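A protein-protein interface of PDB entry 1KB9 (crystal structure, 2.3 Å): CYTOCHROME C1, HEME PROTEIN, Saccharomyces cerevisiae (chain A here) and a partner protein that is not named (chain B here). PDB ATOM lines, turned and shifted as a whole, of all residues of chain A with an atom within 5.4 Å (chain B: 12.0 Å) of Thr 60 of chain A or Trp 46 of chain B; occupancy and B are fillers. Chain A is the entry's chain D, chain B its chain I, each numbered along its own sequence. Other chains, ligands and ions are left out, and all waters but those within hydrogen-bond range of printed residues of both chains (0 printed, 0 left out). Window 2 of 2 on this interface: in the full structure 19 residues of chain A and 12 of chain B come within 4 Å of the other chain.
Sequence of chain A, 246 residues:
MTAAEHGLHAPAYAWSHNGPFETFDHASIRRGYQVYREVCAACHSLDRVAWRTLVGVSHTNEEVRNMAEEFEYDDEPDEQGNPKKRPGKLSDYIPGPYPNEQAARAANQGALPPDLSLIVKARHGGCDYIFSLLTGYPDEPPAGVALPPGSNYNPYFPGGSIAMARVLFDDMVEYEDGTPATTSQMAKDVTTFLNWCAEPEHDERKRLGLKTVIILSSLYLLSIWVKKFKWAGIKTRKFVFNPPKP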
ATOM      1  N   HIS A  26      -6.691  16.587   7.357  1.00  0.00           N
ATOM      2  CA  HIS A  26      -6.606  15.472   8.288  1.00  0.00           C
ATOM      3  C   HIS A  26      -5.278  15.219   8.989  1.00  0.00           C
ATOM      4  O   HIS A  26      -5.254  14.621  10.067  1.00  0.00           O
ATOM      5  CB  HIS A  26      -7.166  14.212   7.642  1.00  0.00           C
ATOM      6  CG  HIS A  26      -8.635  14.298   7.368  1.00  0.00           C
ATOM      7  ND1 HIS A  26      -9.575  13.647   8.136  1.00  0.00           N
ATOM      8  CD2 HIS A  26      -9.329  15.003   6.442  1.00  0.00           C
ATOM      9  CE1 HIS A  26     -10.784  13.949   7.696  1.00  0.00           C
ATOM     10  NE2 HIS A  26     -10.661  14.770   6.670  1.00  0.00           N
ATOM     11  N   ARG A  30      -4.771  14.904  12.992  1.00  0.00           N
ATOM     12  CA  ARG A  30      -3.925  13.884  13.620  1.00  0.00           C
ATOM     13  C   ARG A  30      -2.972  14.513  14.637  1.00  0.00           C
ATOM     14  O   ARG A  30      -2.921  14.092  15.788  1.00  0.00           O
ATOM     15  CB  ARG A  30      -3.137  13.112  12.556  1.00  0.00           C
ATOM     16  CG  ARG A  30      -2.316  11.961  13.115  1.00  0.00           C
ATOM     17  CD  ARG A  30      -1.737  11.094  12.001  1.00  0.00           C
ATOM     18  NE  ARG A  30      -0.814  10.087  12.520  1.00  0.00           N
ATOM     19  CZ  ARG A  30      -1.158   8.855  12.886  1.00  0.00           C
ATOM     20  NH1 ARG A  30      -0.234   8.023  13.345  1.00  0.00           N
ATOM     21  NH2 ARG A  30      -2.415   8.444  12.791  1.00  0.00           N
ATOM     22  N   VAL A  55     -11.246   6.628  13.937  1.00  0.00           N
ATOM     23  CA  VAL A  55     -10.918   5.702  12.860  1.00  0.00           C
ATOM     24  C   VAL A  55     -11.332   6.215  11.491  1.00  0.00           C
ATOM     25  O   VAL A  55     -12.494   6.550  11.263  1.00  0.00           O
ATOM     26  CB  VAL A  55     -11.556   4.327  13.103  1.00  0.00           C
ATOM     27  CG1 VAL A  55     -11.282   3.394  11.930  1.00  0.00           C
ATOM     28  CG2 VAL A  55     -11.026   3.737  14.394  1.00  0.00           C
ATOM     29  N   GLY A  56     -10.370   6.272  10.580  1.00  0.00           N
ATOM     30  CA  GLY A  56     -10.652   6.736   9.238  1.00  0.00           C
ATOM     31  C   GLY A  56     -10.645   8.243   9.119  1.00  0.00           C
ATOM     32  O   GLY A  56     -10.891   8.778   8.034  1.00  0.00           O
ATOM     33  N   VAL A  57     -10.400   8.931  10.233  1.00  0.00           N
ATOM     34  CA  VAL A  57     -10.359  10.387  10.225  1.00  0.00           C
ATOM     35  C   VAL A  57      -8.942  10.879  10.440  1.00  0.00           C
ATOM     36  O   VAL A  57      -8.398  11.615   9.614  1.00  0.00           O
ATOM     37  CB  VAL A  57     -11.264  11.012  11.323  1.00  0.00           C
ATOM     38  CG1 VAL A  57     -11.087  12.531  11.351  1.00  0.00           C
ATOM     39  CG2 VAL A  57     -12.718  10.657  11.070  1.00  0.00           C
ATOM     40  N   SER A  58      -8.350  10.457  11.552  1.00  0.00           N
ATOM     41  CA  SER A  58      -7.002  10.863  11.911  1.00  0.00           C
ATOM     42  C   SER A  58      -6.091   9.683  12.273  1.00  0.00           C
ATOM     43  O   SER A  58      -4.871   9.817  12.264  1.00  0.00           O
ATOM     44  CB  SER A  58      -7.069  11.837  13.085  1.00  0.00           C
ATOM     45  OG  SER A  58      -7.733  11.244  14.184  1.00  0.00           O
ATOM     46  N   HIS A  59      -6.691   8.543  12.606  1.00  0.00           N
ATOM     47  CA  HIS A  59      -5.946   7.348  12.983  1.00  0.00           C
ATOM     48  C   HIS A  59      -6.522   6.087  12.341  1.00  0.00           C
ATOM     49  O   HIS A  59      -7.622   6.102  11.787  1.00  0.00           O
ATOM     50  CB  HIS A  59      -5.954   7.178  14.503  1.00  0.00           C
ATOM     51  CG  HIS A  59      -5.274   8.285  15.244  1.00  0.00           C
ATOM     52  ND1 HIS A  59      -5.690   9.597  15.170  1.00  0.00           N
ATOM     53  CD2 HIS A  59      -4.226   8.272  16.100  1.00  0.00           C
ATOM     54  CE1 HIS A  59      -4.933  10.342  15.953  1.00  0.00           C
ATOM     55  NE2 HIS A  59      -4.036   9.563  16.530  1.00  0.00           N
ATOM     56  N   THR A  60      -5.765   4.998  12.414  1.00  0.00           N
ATOM     57  CA  THR A  60      -6.200   3.720  11.858  1.00  0.00           C
ATOM     58  C   THR A  60      -6.991   2.956  12.917  1.00  0.00           C
ATOM     59  O   THR A  60      -6.913   3.258  14.113  1.00  0.00           O
ATOM     60  CB  THR A  60      -4.998   2.840  11.416  1.00  0.00           C
ATOM     61  OG1 THR A  60      -4.189   2.525  12.557  1.00  0.00           O
ATOM     62  CG2 THR A  60      -4.143   3.563  10.386  1.00  0.00           C
ATOM     63  N   ASN A  61      -7.715   1.937  12.477  1.00  0.00           N
ATOM     64  CA  ASN A  61      -8.504   1.123  13.386  1.00  0.00           C
ATOM     65  C   ASN A  61      -7.629   0.530  14.491  1.00  0.00           C
ATOM     66  O   ASN A  61      -8.047   0.445  15.647  1.00  0.00           O
ATOM     67  CB  ASN A  61      -9.211   0.009  12.611  1.00  0.00           C
ATOM     68  CG  ASN A  61     -10.248  -0.704  13.446  1.00  0.00           C
ATOM     69  OD1 ASN A  61      -9.914  -1.536  14.294  1.00  0.00           O
ATOM     70  ND2 ASN A  61     -11.519  -0.364  13.232  1.00  0.00           N
ATOM     71  N   GLU A  62      -6.402   0.156  14.130  1.00  0.00           N
ATOM     72  CA  GLU A  62      -5.447  -0.431  15.070  1.00  0.00           C
ATOM     73  C   GLU A  62      -4.943   0.578  16.097  1.00  0.00           C
ATOM     74  O   GLU A  62      -4.929   0.290  17.299  1.00  0.00           O
ATOM     75  CB  GLU A  62      -4.253  -1.044  14.323  1.00  0.00           C
ATOM     76  CG  GLU A  62      -4.591  -2.247  13.428  1.00  0.00           C
ATOM     77  CD  GLU A  62      -5.412  -1.880  12.193  1.00  0.00           C
ATOM     78  OE1 GLU A  62      -5.124  -0.839  11.560  1.00  0.00           O
ATOM     79  OE2 GLU A  62      -6.344  -2.644  11.852  1.00  0.00           O
ATOM     80  N   GLU A  63      -4.537   1.757  15.620  1.00  0.00           N
ATOM     81  CA  GLU A  63      -4.033   2.821  16.492  1.00  0.00           C
ATOM     82  C   GLU A  63      -5.038   3.241  17.558  1.00  0.00           C
ATOM     83  O   GLU A  63      -4.672   3.450  18.715  1.00  0.00           O
ATOM     84  CB  GLU A  63      -3.649   4.050  15.677  1.00  0.00           C
ATOM     85  CG  GLU A  63      -2.510   3.836  14.716  1.00  0.00           C
ATOM     86  CD  GLU A  63      -2.104   5.117  14.031  1.00  0.00           C
ATOM     87  OE1 GLU A  63      -1.154   5.768  14.517  1.00  0.00           O
ATOM     88  OE2 GLU A  63      -2.739   5.481  13.019  1.00  0.00           O
ATOM     89  N   VAL A  64      -6.301   3.381  17.158  1.00  0.00           N
ATOM     90  CA  VAL A  64      -7.347   3.781  18.089  1.00  0.00           C
ATOM     91  C   VAL A  64      -7.590   2.703  19.136  1.00  0.00           C
ATOM     92  O   VAL A  64      -7.780   3.008  20.315  1.00  0.00           O
ATOM     93  CB  VAL A  64      -8.672   4.122  17.354  1.00  0.00           C
ATOM     94  CG1 VAL A  64      -9.760   4.474  18.349  1.00  0.00           C
ATOM     95  CG2 VAL A  64      -8.454   5.283  16.406  1.00  0.00           C
ATOM     96  N   ARG A  65      -7.558   1.441  18.713  1.00  0.00           N
ATOM     97  CA  ARG A  65      -7.778   0.342  19.644  1.00  0.00           C
ATOM     98  C   ARG A  65      -6.711   0.333  20.735  1.00  0.00           C
ATOM     99  O   ARG A  65      -7.032   0.165  21.912  1.00  0.00           O
ATOM    100  CB  ARG A  65      -7.830  -1.001  18.911  1.00  0.00           C
ATOM    101  CG  ARG A  65      -8.161  -2.176  19.826  1.00  0.00           C
ATOM    102  CD  ARG A  65      -8.457  -3.448  19.046  1.00  0.00           C
ATOM    103  NE  ARG A  65      -9.776  -3.414  18.410  1.00  0.00           N
ATOM    104  CZ  ARG A  65      -9.982  -3.386  17.093  1.00  0.00           C
ATOM    105  NH1 ARG A  65     -11.223  -3.358  16.617  1.00  0.00           N
ATOM    106  NH2 ARG A  65      -8.952  -3.380  16.252  1.00  0.00           N
ATOM    107  N   THR B  34     -18.206  13.521  -6.208  1.00  0.00           N
ATOM    108  CA  THR B  34     -17.248  12.957  -5.260  1.00  0.00           C
ATOM    109  C   THR B  34     -15.830  13.027  -5.835  1.00  0.00           C
ATOM    110  O   THR B  34     -14.877  13.362  -5.125  1.00  0.00           O
ATOM    111  CB  THR B  34     -17.570  11.489  -4.927  1.00  0.00           C
ATOM    112  OG1 THR B  34     -18.868  11.402  -4.324  1.00  0.00           O
ATOM    113  CG2 THR B  34     -16.526  10.922  -3.967  1.00  0.00           C
ATOM    114  N   TYR B  37     -14.638  16.665  -5.836  1.00  0.00           N
ATOM    115  CA  TYR B  37     -14.447  17.045  -4.439  1.00  0.00           C
ATOM    116  C   TYR B  37     -13.155  16.488  -3.843  1.00  0.00           C
ATOM    117  O   TYR B  37     -12.373  17.237  -3.252  1.00  0.00           O
ATOM    118  CB  TYR B  37     -15.658  16.598  -3.609  1.00  0.00           C
ATOM    119  CG  TYR B  37     -15.746  17.195  -2.221  1.00  0.00           C
ATOM    120  CD1 TYR B  37     -16.032  18.555  -2.037  1.00  0.00           C
ATOM    121  CD2 TYR B  37     -15.592  16.395  -1.088  1.00  0.00           C
ATOM    122  CE1 TYR B  37     -16.163  19.099  -0.759  1.00  0.00           C
ATOM    123  CE2 TYR B  37     -15.724  16.925   0.193  1.00  0.00           C
ATOM    124  CZ  TYR B  37     -16.007  18.275   0.349  1.00  0.00           C
ATOM    125  OH  TYR B  37     -16.121  18.795   1.613  1.00  0.00           O
ATOM    126  N   GLU B  38     -12.943  15.182  -3.985  1.00  0.00           N
ATOM    127  CA  GLU B  38     -11.739  14.541  -3.450  1.00  0.00           C
ATOM    128  C   GLU B  38     -10.455  15.028  -4.130  1.00  0.00           C
ATOM    129  O   GLU B  38      -9.408  15.130  -3.491  1.00  0.00           O
ATOM    130  CB  GLU B  38     -11.838  13.021  -3.553  1.00  0.00           C
ATOM    131  CG  GLU B  38     -12.896  12.420  -2.666  1.00  0.00           C
ATOM    132  CD  GLU B  38     -12.755  10.920  -2.524  1.00  0.00           C
ATOM    133  OE1 GLU B  38     -13.011  10.412  -1.410  1.00  0.00           O
ATOM    134  OE2 GLU B  38     -12.390  10.247  -3.518  1.00  0.00           O
ATOM    135  N   ASN B  39     -10.548  15.325  -5.423  1.00  0.00           N
ATOM    136  CA  ASN B  39      -9.411  15.820  -6.184  1.00  0.00           C
ATOM    137  C   ASN B  39      -9.077  17.244  -5.744  1.00  0.00           C
ATOM    138  O   ASN B  39      -7.908  17.587  -5.551  1.00  0.00           O
ATOM    139  CB  ASN B  39      -9.722  15.795  -7.684  1.00  0.00           C
ATOM    140  CG  ASN B  39      -8.559  16.287  -8.526  1.00  0.00           C
ATOM    141  OD1 ASN B  39      -7.536  15.609  -8.647  1.00  0.00           O
ATOM    142  ND2 ASN B  39      -8.699  17.484  -9.091  1.00  0.00           N
ATOM    143  N   HIS B  40     -10.107  18.072  -5.590  1.00  0.00           N
ATOM    144  CA  HIS B  40      -9.924  19.458  -5.161  1.00  0.00           C
ATOM    145  C   HIS B  40      -9.253  19.519  -3.789  1.00  0.00           C
ATOM    146  O   HIS B  40      -8.539  20.469  -3.489  1.00  0.00           O
ATOM    147  CB  HIS B  40     -11.275  20.202  -5.119  1.00  0.00           C
ATOM    148  CG  HIS B  40     -11.166  21.629  -4.669  1.00  0.00           C
ATOM    149  ND1 HIS B  40     -10.986  22.676  -5.549  1.00  0.00           N
ATOM    150  CD2 HIS B  40     -11.159  22.176  -3.429  1.00  0.00           C
ATOM    151  CE1 HIS B  40     -10.865  23.803  -4.871  1.00  0.00           C
ATOM    152  NE2 HIS B  40     -10.967  23.525  -3.583  1.00  0.00           N
ATOM    153  N   ASN B  41      -9.486  18.500  -2.966  1.00  0.00           N
ATOM    154  CA  ASN B  41      -8.908  18.442  -1.625  1.00  0.00           C
ATOM    155  C   ASN B  41      -7.752  17.457  -1.468  1.00  0.00           C
ATOM    156  O   ASN B  41      -7.475  16.979  -0.365  1.00  0.00           O
ATOM    157  CB  ASN B  41      -9.998  18.138  -0.594  1.00  0.00           C
ATOM    158  CG  ASN B  41     -10.839  19.354  -0.272  1.00  0.00           C
ATOM    159  OD1 ASN B  41     -10.526  20.107   0.650  1.00  0.00           O
ATOM    160  ND2 ASN B  41     -11.901  19.568  -1.046  1.00  0.00           N
ATOM    161  N   LYS B  42      -7.061  17.188  -2.574  1.00  0.00           N
ATOM    162  CA  LYS B  42      -5.926  16.272  -2.589  1.00  0.00           C
ATOM    163  C   LYS B  42      -4.858  16.737  -1.593  1.00  0.00           C
ATOM    164  O   LYS B  42      -4.509  17.916  -1.542  1.00  0.00           O
ATOM    165  CB  LYS B  42      -5.339  16.198  -4.004  1.00  0.00           C
ATOM    166  CG  LYS B  42      -4.400  15.023  -4.236  1.00  0.00           C
ATOM    167  CD  LYS B  42      -3.661  15.156  -5.568  1.00  0.00           C
ATOM    168  CE  LYS B  42      -4.605  15.074  -6.772  1.00  0.00           C
ATOM    169  NZ  LYS B  42      -5.246  13.728  -6.918  1.00  0.00           N
ATOM    170  N   GLY B  43      -4.385  15.806  -0.774  1.00  0.00           N
ATOM    171  CA  GLY B  43      -3.377  16.126   0.217  1.00  0.00           C
ATOM    172  C   GLY B  43      -3.933  16.273   1.619  1.00  0.00           C
ATOM    173  O   GLY B  43      -3.258  15.947   2.596  1.00  0.00           O
ATOM    174  N   LYS B  44      -5.178  16.736   1.717  1.00  0.00           N
ATOM    175  CA  LYS B  44      -5.834  16.954   3.003  1.00  0.00           C
ATOM    176  C   LYS B  44      -6.619  15.758   3.511  1.00  0.00           C
ATOM    177  O   LYS B  44      -6.801  15.601   4.720  1.00  0.00           O
ATOM    178  CB  LYS B  44      -6.746  18.173   2.907  1.00  0.00           C
ATOM    179  CG  LYS B  44      -5.996  19.478   2.739  1.00  0.00           C
ATOM    180  CD  LYS B  44      -6.792  20.500   1.935  1.00  0.00           C
ATOM    181  CE  LYS B  44      -8.057  20.938   2.641  1.00  0.00           C
ATOM    182  NZ  LYS B  44      -8.816  21.920   1.819  1.00  0.00           N
ATOM    183  N   LEU B  45      -7.069  14.913   2.588  1.00  0.00           N
ATOM    184  CA  LEU B  45      -7.853  13.720   2.922  1.00  0.00           C
ATOM    185  C   LEU B  45      -7.111  12.677   3.748  1.00  0.00           C
ATOM    186  O   LEU B  45      -5.881  12.639   3.768  1.00  0.00           O
ATOM    187  CB  LEU B  45      -8.370  13.056   1.643  1.00  0.00           C
ATOM    188  CG  LEU B  45      -9.686  13.516   1.010  1.00  0.00           C
ATOM    189  CD1 LEU B  45     -10.090  14.906   1.487  1.00  0.00           C
ATOM    190  CD2 LEU B  45      -9.554  13.464  -0.509  1.00  0.00           C
ATOM    191  N   TRP B  46      -7.875  11.837   4.436  1.00  0.00           N
ATOM    192  CA  TRP B  46      -7.303  10.762   5.241  1.00  0.00           C
ATOM    193  C   TRP B  46      -6.613   9.731   4.334  1.00  0.00           C
ATOM    194  O   TRP B  46      -5.648   9.093   4.747  1.00  0.00           O
ATOM    195  CB  TRP B  46      -8.388  10.077   6.073  1.00  0.00           C
ATOM    196  CG  TRP B  46      -7.929   8.800   6.705  1.00  0.00           C
ATOM    197  CD1 TRP B  46      -8.422   7.546   6.476  1.00  0.00           C
ATOM    198  CD2 TRP B  46      -6.870   8.647   7.658  1.00  0.00           C
ATOM    199  NE1 TRP B  46      -7.736   6.623   7.229  1.00  0.00           N
ATOM    200  CE2 TRP B  46      -6.779   7.272   7.964  1.00  0.00           C
ATOM    201  CE3 TRP B  46      -5.988   9.541   8.282  1.00  0.00           C
ATOM    202  CZ2 TRP B  46      -5.843   6.766   8.870  1.00  0.00           C
ATOM    203  CZ3 TRP B  46      -5.057   9.040   9.182  1.00  0.00           C
ATOM    204  CH2 TRP B  46      -4.991   7.663   9.467  1.00  0.00           C
ATOM    205  N   LYS B  47      -7.133   9.558   3.118  1.00  0.00           N
ATOM    206  CA  LYS B  47      -6.564   8.623   2.145  1.00  0.00           C
ATOM    207  C   LYS B  47      -5.120   9.013   1.883  1.00  0.00           C
ATOM    208  O   LYS B  47      -4.237   8.161   1.796  1.00  0.00           O
ATOM    209  CB  LYS B  47      -7.298   8.693   0.803  1.00  0.00           C
ATOM    210  CG  LYS B  47      -8.786   8.412   0.831  1.00  0.00           C
ATOM    211  CD  LYS B  47      -9.332   8.290  -0.595  1.00  0.00           C
ATOM    212  CE  LYS B  47      -8.932   9.487  -1.467  1.00  0.00           C
ATOM    213  NZ  LYS B  47      -9.414   9.364  -2.880  1.00  0.00           N
ATOM    214  N   ASP B  48      -4.903  10.317   1.741  1.00  0.00           N
ATOM    215  CA  ASP B  48      -3.591  10.875   1.470  1.00  0.00           C
ATOM    216  C   ASP B  48      -2.675  10.793   2.681  1.00  0.00           C
ATOM    217  O   ASP B  48      -1.486  10.515   2.548  1.00  0.00           O
ATOM    218  CB  ASP B  48      -3.734  12.323   1.002  1.00  0.00           C
ATOM    219  CG  ASP B  48      -4.728  12.470  -0.140  1.00  0.00           C
ATOM    220  OD1 ASP B  48      -5.473  13.471  -0.162  1.00  0.00           O
ATOM    221  OD2 ASP B  48      -4.782  11.576  -1.014  1.00  0.00           O
ATOM    222  N   VAL B  49      -3.236  11.016   3.863  1.00  0.00           N
ATOM    223  CA  VAL B  49      -2.459  10.963   5.093  1.00  0.00           C
ATOM    224  C   VAL B  49      -2.030   9.534   5.426  1.00  0.00           C
ATOM    225  O   VAL B  49      -0.928   9.319   5.934  1.00  0.00           O
ATOM    226  CB  VAL B  49      -3.247  11.567   6.277  1.00  0.00           C
ATOM    227  CG1 VAL B  49      -2.439  11.474   7.564  1.00  0.00           C
ATOM    228  CG2 VAL B  49      -3.594  13.013   5.979  1.00  0.00           C
ATOM    229  N   LYS B  50      -2.885   8.562   5.113  1.00  0.00           N
ATOM    230  CA  LYS B  50      -2.580   7.161   5.392  1.00  0.00           C
ATOM    231  C   LYS B  50      -1.426   6.652   4.526  1.00  0.00           C
ATOM    232  O   LYS B  50      -0.676   5.764   4.937  1.00  0.00           O
ATOM    233  CB  LYS B  50      -3.816   6.282   5.192  1.00  0.00           C
ATOM    234  CG  LYS B  50      -3.640   4.872   5.740  1.00  0.00           C
ATOM    235  CD  LYS B  50      -4.869   4.004   5.535  1.00  0.00           C
ATOM    236  CE  LYS B  50      -4.657   2.625   6.158  1.00  0.00           C
ATOM    237  NZ  LYS B  50      -5.839   1.732   6.003  1.00  0.00           N
ATOM    238  N   ALA B  51      -1.292   7.225   3.331  1.00  0.00           N
ATOM    239  CA  ALA B  51      -0.230   6.853   2.398  1.00  0.00           C
ATOM    240  C   ALA B  51       1.139   7.268   2.943  1.00  0.00           C
ATOM    241  O   ALA B  51       2.140   6.577   2.735  1.00  0.00           O
ATOM    242  CB  ALA B  51      -0.479   7.495   1.034  1.00  0.00           C
ATOM    243  N   ARG B  52       1.164   8.381   3.672  1.00  0.00           N
ATOM    244  CA  ARG B  52       2.394   8.899   4.264  1.00  0.00           C
ATOM    245  C   ARG B  52       2.687   8.249   5.616  1.00  0.00           C
ATOM    246  O   ARG B  52       3.617   8.650   6.314  1.00  0.00           O
ATOM    247  CB  ARG B  52       2.302  10.418   4.435  1.00  0.00           C
ATOM    248  CG  ARG B  52       1.834  11.165   3.193  1.00  0.00           C
ATOM    249  CD  ARG B  52       2.778  12.301   2.834  1.00  0.00           C
ATOM    250  NE  ARG B  52       4.058  11.806   2.332  1.00  0.00           N
ATOM    251  CZ  ARG B  52       5.248  12.223   2.754  1.00  0.00           C
ATOM    252  NH1 ARG B  52       5.338  13.151   3.699  1.00  0.00           N
ATOM    253  NH2 ARG B  52       6.353  11.704   2.236  1.00  0.00           N
ATOM    254  N   ILE B  53       1.878   7.259   5.988  1.00  0.00           N
ATOM    255  CA  ILE B  53       2.042   6.544   7.255  1.00  0.00           C
ATOM    256  C   ILE B  53       2.316   5.063   6.990  1.00  0.00           C
ATOM    257  O   ILE B  53       1.796   4.487   6.033  1.00  0.00           O
ATOM    258  CB  ILE B  53       0.776   6.684   8.154  1.00  0.00           C
ATOM    259  CG1 ILE B  53       0.530   8.156   8.510  1.00  0.00           C
ATOM    260  CG2 ILE B  53       0.917   5.853   9.430  1.00  0.00           C
ATOM    261  CD1 ILE B  53       1.660   8.815   9.285  1.00  0.00           C
ATOM    262  N   ALA B  54       3.144   4.459   7.840  1.00  0.00           N
ATOM    263  CA  ALA B  54       3.496   3.046   7.714  1.00  0.00           C
ATOM    264  C   ALA B  54       3.725   2.420   9.090  1.00  0.00           C
ATOM    265  O   ALA B  54       4.730   2.692   9.753  1.00  0.00           O
ATOM    266  CB  ALA B  54       4.741   2.885   6.841  1.00  0.00           C
ATOM    267  N   ALA B  55       2.780   1.580   9.509  1.00  0.00           N
ATOM    268  CA  ALA B  55       2.853   0.907  10.803  1.00  0.00           C
ATOM    269  C   ALA B  55       2.234  -0.492  10.748  1.00  0.00           C
ATOM    270  O   ALA B  55       2.312  -1.210  11.770  1.00  0.00           O
ATOM    271  CB  ALA B  55       2.164   1.757  11.878  1.00  0.00           C
ATOM    272  OXT ALA B  55       1.683  -0.861   9.686  1.00  0.00           O
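Hydrophobic or aromatic side chains of chain B within 4 Å of the printed part of chain A: Trp 46. Of the 13 printed residues of chain A, 6 touch a printed residue of chain B. Hydrophobic or aromatic side chains of chain A within 4 Å of the printed part of chain B: His 26.
The backbone carbonyl oxygen of Val 57 of chain A sits at hydrogen-bond distance from a ring nitrogen (ND1) of His 26 of chain A (2.8 Å). The side-chain carboxylate (OE2) of Glu 63 of chain A lies within hydrogen-bond range of the backbone NH (N) of Thr 60 of chain A (3.1 Å). The side-chain amino group of Lys 44 of chain B is in hydrogen-bond range of the side-chain amide oxygen of Asn 41 of chain B. A ring nitrogen (ND1) of His 59 of chain A lies within hydrogen-bond range of the side-chain hydroxyl (OG) of Ser 58 of chain A. The guanidinium group (NH2) of Arg 30 of chain A sits at hydrogen-bond distance from the backbone carbonyl oxygen (O) of Ser 58 of chain A, at 2.9 Å.
N of Trp 46 of chain B touches CG of His 26 of chain A, 3.9 Å away. O of Gly 56 of chain A touches CD1 of Trp 46 of chain B (3.2 Å). CE3 of Trp 46 of chain B touches O of Val 57 of chain A (3.4 Å). O of Ser 58 of chain A touches CZ3 of Trp 46 of chain B (3.2 Å). His 59 of chain A touches Trp 46 of chain B (O to CZ2, 3.5 Å). Thr 60 of chain A touches Trp 46 of chain B (CG2 to CZ2, 3.9 Å).
N of His 26 of chain A sits at hydrogen-bond distance from O of Lys 44 of chain B.
His 26 of chain A touches just these residues of chain B: Lys 44 and Trp 46. No residue of chain B comes within 4 Å of Val 55 of chain A. Printed residues of chain B within 4 Å of Gly 56 of chain A: Trp 46. Of chain B, only Trp 46 (3.4 Å) comes within 4 Å of Val 57 of chain A. Of chain B, only Trp 46 (3.2 Å) comes within 4 Å of Ser 58 of chain A. Of chain B, only Trp 46 (3.5 Å) comes within 4 Å of His 59 of chain A. No residue of chain B comes within 4 Å of Glu 62 of chain A. No residue of chain B comes within 4 Å of Glu 63 of chain A. Thr 34 of chain B touches none of the printed residues of chain A. Gly 43 of chain B touches none of the printed residues of chain A. Printed residues of chain A within 4 Å of Lys 44 of chain B: His 26 (2.8 Å). The nearest residue of chain B that does not touch Thr 60 of chain A is Lys 50 of chain B (4.4 Å). The nearest residue of chain A that does not touch Trp 46 of chain B is Arg 30 of chain A (4.3 Å).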
